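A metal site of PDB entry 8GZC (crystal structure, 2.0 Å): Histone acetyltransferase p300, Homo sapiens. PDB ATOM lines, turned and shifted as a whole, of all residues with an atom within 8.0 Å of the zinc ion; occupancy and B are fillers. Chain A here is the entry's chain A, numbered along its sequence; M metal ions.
The zinc ion is bound by ND1 of His 99, at 2.1 Å.
The zinc ion is bound by SG of Cys 7 (2.3 Å).
The zinc ion is bound by SG of Cys 8 (2.3 Å).
SG of Cys 102 is bound to the zinc ion (2.3 Å).
The zinc ion has four donor atoms within binding distance.
The side-chain sulfur (SG) of Cys 102 lies close to the guanidinium group (NH2) of Arg 433.
SG of Cys 8 sits close to N of Arg 10.
Within 4 Å of the zinc ion: Cys 7, Cys 8, His 99 and Cys 102.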
ATOM      1  N   TYR A   6      -9.741  10.987  -5.654  1.00  0.00           N
ATOM      2  CA  TYR A   6     -10.833  11.913  -5.925  1.00  0.00           C
ATOM      3  C   TYR A   6     -10.297  13.314  -6.184  1.00  0.00           C
ATOM      4  O   TYR A   6      -9.094  13.548  -6.126  1.00  0.00           O
ATOM      5  CB  TYR A   6     -11.819  11.923  -4.752  1.00  0.00           C
ATOM      6  N   CYS A   7     -11.203  14.261  -6.504  1.00  0.00           N
ATOM      7  CA  CYS A   7     -10.801  15.649  -6.750  1.00  0.00           C
ATOM      8  C   CYS A   7     -10.680  16.437  -5.462  1.00  0.00           C
ATOM      9  O   CYS A   7      -9.577  16.735  -4.982  1.00  0.00           O
ATOM     10  CB  CYS A   7     -11.837  16.342  -7.631  1.00  0.00           C
ATOM     11  SG  CYS A   7     -13.423  15.465  -7.663  1.00  0.00           S
ATOM     12  N   CYS A   8     -11.830  16.714  -4.857  1.00  0.00           N
ATOM     13  CA  CYS A   8     -11.916  17.384  -3.580  1.00  0.00           C
ATOM     14  C   CYS A   8     -11.331  16.534  -2.479  1.00  0.00           C
ATOM     15  O   CYS A   8     -11.123  17.038  -1.371  1.00  0.00           O
ATOM     16  CB  CYS A   8     -13.389  17.683  -3.298  1.00  0.00           C
ATOM     17  SG  CYS A   8     -14.487  16.367  -3.937  1.00  0.00           S
ATOM     18  N   GLY A   9     -11.059  15.263  -2.759  1.00  0.00           N
ATOM     19  CA  GLY A   9     -10.712  14.319  -1.732  1.00  0.00           C
ATOM     20  C   GLY A   9     -11.851  14.125  -0.763  1.00  0.00           C
ATOM     21  O   GLY A   9     -11.623  13.936   0.442  1.00  0.00           O
ATOM     22  N   ARG A  10     -13.092  14.173  -1.256  1.00  0.00           N
ATOM     23  CA  ARG A  10     -14.266  14.139  -0.411  1.00  0.00           C
ATOM     24  C   ARG A  10     -15.118  12.927  -0.757  1.00  0.00           C
ATOM     25  O   ARG A  10     -15.347  12.637  -1.932  1.00  0.00           O
ATOM     26  CB  ARG A  10     -15.087  15.417  -0.536  1.00  0.00           C
ATOM     27  CG  ARG A  10     -14.715  16.473   0.499  1.00  0.00           C
ATOM     28  CD  ARG A  10     -15.888  17.377   0.821  1.00  0.00           C
ATOM     29  NE  ARG A  10     -16.338  18.114  -0.360  1.00  0.00           N
ATOM     30  CZ  ARG A  10     -17.474  18.785  -0.422  1.00  0.00           C
ATOM     31  NH1 ARG A  10     -18.312  18.847   0.597  1.00  0.00           N
ATOM     32  NH2 ARG A  10     -17.779  19.431  -1.550  1.00  0.00           N
ATOM     33  N   LYS A  11     -15.567  12.219   0.279  1.00  0.00           N
ATOM     34  CA  LYS A  11     -16.493  11.102   0.135  1.00  0.00           C
ATOM     35  C   LYS A  11     -17.906  11.684   0.069  1.00  0.00           C
ATOM     36  O   LYS A  11     -18.486  12.045   1.090  1.00  0.00           O
ATOM     37  CB  LYS A  11     -16.341  10.123   1.293  1.00  0.00           C
ATOM     38  CG  LYS A  11     -16.797   8.716   0.996  1.00  0.00           C
ATOM     39  CD  LYS A  11     -17.542   8.122   2.178  1.00  0.00           C
ATOM     40  CE  LYS A  11     -18.337   6.897   1.775  1.00  0.00           C
ATOM     41  NZ  LYS A  11     -17.491   5.917   1.046  1.00  0.00           N
ATOM     42  N   LEU A  12     -18.448  11.782  -1.142  1.00  0.00           N
ATOM     43  CA  LEU A  12     -19.702  12.474  -1.384  1.00  0.00           C
ATOM     44  C   LEU A  12     -20.800  11.492  -1.767  1.00  0.00           C
ATOM     45  O   LEU A  12     -20.574  10.585  -2.583  1.00  0.00           O
ATOM     46  CB  LEU A  12     -19.534  13.518  -2.491  1.00  0.00           C
ATOM     47  CG  LEU A  12     -18.679  14.749  -2.168  1.00  0.00           C
ATOM     48  CD1 LEU A  12     -18.421  15.561  -3.432  1.00  0.00           C
ATOM     49  CD2 LEU A  12     -19.340  15.613  -1.103  1.00  0.00           C
ATOM     50  N   GLU A  86     -22.185   9.743  -5.101  1.00  0.00           N
ATOM     51  CA  GLU A  86     -22.036  10.580  -6.273  1.00  0.00           C
ATOM     52  C   GLU A  86     -21.288   9.826  -7.367  1.00  0.00           C
ATOM     53  O   GLU A  86     -20.435   8.982  -7.107  1.00  0.00           O
ATOM     54  CB  GLU A  86     -21.293  11.879  -5.927  1.00  0.00           C
ATOM     55  CG  GLU A  86     -22.147  12.899  -5.193  1.00  0.00           C
ATOM     56  CD  GLU A  86     -21.724  14.323  -5.488  1.00  0.00           C
ATOM     57  OE1 GLU A  86     -20.957  14.524  -6.465  1.00  0.00           O
ATOM     58  OE2 GLU A  86     -22.148  15.236  -4.761  1.00  0.00           O
ATOM     59  N   LEU A  87     -21.632  10.128  -8.616  1.00  0.00           N
ATOM     60  CA  LEU A  87     -21.005   9.468  -9.746  1.00  0.00           C
ATOM     61  C   LEU A  87     -19.664  10.115 -10.075  1.00  0.00           C
ATOM     62  O   LEU A  87     -19.443  11.316  -9.856  1.00  0.00           O
ATOM     63  CB  LEU A  87     -21.905   9.534 -10.975  1.00  0.00           C
ATOM     64  CG  LEU A  87     -23.330   9.004 -10.767  1.00  0.00           C
ATOM     65  CD1 LEU A  87     -24.026   8.836 -12.104  1.00  0.00           C
ATOM     66  CD2 LEU A  87     -23.291   7.675 -10.014  1.00  0.00           C
ATOM     67  N   PHE A  88     -18.750   9.306 -10.599  1.00  0.00           N
ATOM     68  CA  PHE A  88     -17.488   9.773 -11.116  1.00  0.00           C
ATOM     69  C   PHE A  88     -17.499   9.711 -12.642  1.00  0.00           C
ATOM     70  O   PHE A  88     -18.305   9.000 -13.248  1.00  0.00           O
ATOM     71  CB  PHE A  88     -16.319   8.944 -10.578  1.00  0.00           C
ATOM     72  CG  PHE A  88     -16.048   9.140  -9.113  1.00  0.00           C
ATOM     73  CD1 PHE A  88     -16.694   8.367  -8.173  1.00  0.00           C
ATOM     74  CD2 PHE A  88     -15.158  10.109  -8.686  1.00  0.00           C
ATOM     75  CE1 PHE A  88     -16.460   8.542  -6.824  1.00  0.00           C
ATOM     76  CE2 PHE A  88     -14.916  10.294  -7.331  1.00  0.00           C
ATOM     77  CZ  PHE A  88     -15.564   9.510  -6.404  1.00  0.00           C
ATOM     78  N   LYS A  97     -10.112   9.823 -12.341  1.00  0.00           N
ATOM     79  CA  LYS A  97     -11.523   9.730 -11.974  1.00  0.00           C
ATOM     80  C   LYS A  97     -11.931  10.996 -11.231  1.00  0.00           C
ATOM     81  O   LYS A  97     -11.259  11.410 -10.293  1.00  0.00           O
ATOM     82  CB  LYS A  97     -11.770   8.492 -11.103  1.00  0.00           C
ATOM     83  N   MET A  98     -13.043  11.597 -11.649  1.00  0.00           N
ATOM     84  CA  MET A  98     -13.473  12.885 -11.112  1.00  0.00           C
ATOM     85  C   MET A  98     -14.974  12.888 -10.870  1.00  0.00           C
ATOM     86  O   MET A  98     -15.739  12.419 -11.712  1.00  0.00           O
ATOM     87  CB  MET A  98     -13.108  14.028 -12.076  1.00  0.00           C
ATOM     88  CG  MET A  98     -11.611  14.226 -12.321  1.00  0.00           C
ATOM     89  SD  MET A  98     -10.838  15.375 -11.163  1.00  0.00           S
ATOM     90  CE  MET A  98     -10.632  14.266  -9.793  1.00  0.00           C
ATOM     91  N   HIS A  99     -15.382  13.437  -9.718  1.00  0.00           N
ATOM     92  CA  HIS A  99     -16.798  13.646  -9.449  1.00  0.00           C
ATOM     93  C   HIS A  99     -17.440  14.367 -10.624  1.00  0.00           C
ATOM     94  O   HIS A  99     -16.946  15.398 -11.079  1.00  0.00           O
ATOM     95  CB  HIS A  99     -16.996  14.483  -8.180  1.00  0.00           C
ATOM     96  CG  HIS A  99     -16.760  13.738  -6.897  1.00  0.00           C
ATOM     97  ND1 HIS A  99     -15.879  14.190  -5.942  1.00  0.00           N
ATOM     98  CD2 HIS A  99     -17.305  12.597  -6.411  1.00  0.00           C
ATOM     99  CE1 HIS A  99     -15.877  13.345  -4.919  1.00  0.00           C
ATOM    100  NE2 HIS A  99     -16.729  12.371  -5.179  1.00  0.00           N
ATOM    101  N   GLN A 100     -18.543  13.805 -11.138  1.00  0.00           N
ATOM    102  CA  GLN A 100     -19.181  14.407 -12.302  1.00  0.00           C
ATOM    103  C   GLN A 100     -19.678  15.805 -11.974  1.00  0.00           C
ATOM    104  O   GLN A 100     -19.555  16.721 -12.805  1.00  0.00           O
ATOM    105  CB  GLN A 100     -20.332  13.534 -12.795  1.00  0.00           C
ATOM    106  CG  GLN A 100     -20.857  13.952 -14.152  1.00  0.00           C
ATOM    107  CD  GLN A 100     -21.941  13.038 -14.679  1.00  0.00           C
ATOM    108  OE1 GLN A 100     -22.599  12.330 -13.915  1.00  0.00           O
ATOM    109  NE2 GLN A 100     -22.145  13.058 -15.993  1.00  0.00           N
ATOM    110  N   ILE A 101     -20.230  16.001 -10.784  1.00  0.00           N
ATOM    111  CA  ILE A 101     -20.736  17.315 -10.383  1.00  0.00           C
ATOM    112  C   ILE A 101     -19.586  18.309 -10.237  1.00  0.00           C
ATOM    113  O   ILE A 101     -19.721  19.490 -10.577  1.00  0.00           O
ATOM    114  CB  ILE A 101     -21.569  17.189  -9.096  1.00  0.00           C
ATOM    115  CG1 ILE A 101     -22.889  16.468  -9.401  1.00  0.00           C
ATOM    116  CG2 ILE A 101     -21.831  18.550  -8.474  1.00  0.00           C
ATOM    117  CD1 ILE A 101     -23.594  15.928  -8.180  1.00  0.00           C
ATOM    118  N   CYS A 102     -18.428  17.847  -9.730  1.00  0.00           N
ATOM    119  CA  CYS A 102     -17.291  18.734  -9.537  1.00  0.00           C
ATOM    120  C   CYS A 102     -16.793  19.319 -10.855  1.00  0.00           C
ATOM    121  O   CYS A 102     -16.531  20.513 -10.957  1.00  0.00           O
ATOM    122  CB  CYS A 102     -16.161  18.000  -8.808  1.00  0.00           C
ATOM    123  SG  CYS A 102     -16.324  17.909  -7.015  1.00  0.00           S
ATOM    124  N   VAL A 103     -16.662  18.470 -11.885  1.00  0.00           N
ATOM    125  CA  VAL A 103     -16.151  18.937 -13.173  1.00  0.00           C
ATOM    126  C   VAL A 103     -17.269  19.331 -14.123  1.00  0.00           C
ATOM    127  O   VAL A 103     -16.974  19.849 -15.214  1.00  0.00           O
ATOM    128  CB  VAL A 103     -15.258  17.874 -13.837  1.00  0.00           C
ATOM    129  CG1 VAL A 103     -14.108  17.499 -12.914  1.00  0.00           C
ATOM    130  CG2 VAL A 103     -16.066  16.650 -14.224  1.00  0.00           C
ATOM    131  N   ARG A 433     -22.087  23.721  -5.721  1.00  0.00           N
ATOM    132  CA  ARG A 433     -21.649  22.791  -6.764  1.00  0.00           C
ATOM    133  C   ARG A 433     -22.811  21.946  -7.280  1.00  0.00           C
ATOM    134  O   ARG A 433     -22.918  21.717  -8.492  1.00  0.00           O
ATOM    135  CB  ARG A 433     -20.515  21.899  -6.237  1.00  0.00           C
ATOM    136  CG  ARG A 433     -20.871  21.071  -5.009  1.00  0.00           C
ATOM    137  CD  ARG A 433     -19.650  20.320  -4.499  1.00  0.00           C
ATOM    138  NE  ARG A 433     -19.211  19.298  -5.448  1.00  0.00           N
ATOM    139  CZ  ARG A 433     -19.769  18.105  -5.571  1.00  0.00           C
ATOM    140  NH1 ARG A 433     -20.810  17.743  -4.843  1.00  0.00           N
ATOM    141  NH2 ARG A 433     -19.270  17.249  -6.471  1.00  0.00           N
HETATM  142 ZN    ZN M   1     -15.065  16.144  -6.174  1.00  0.00          ZN
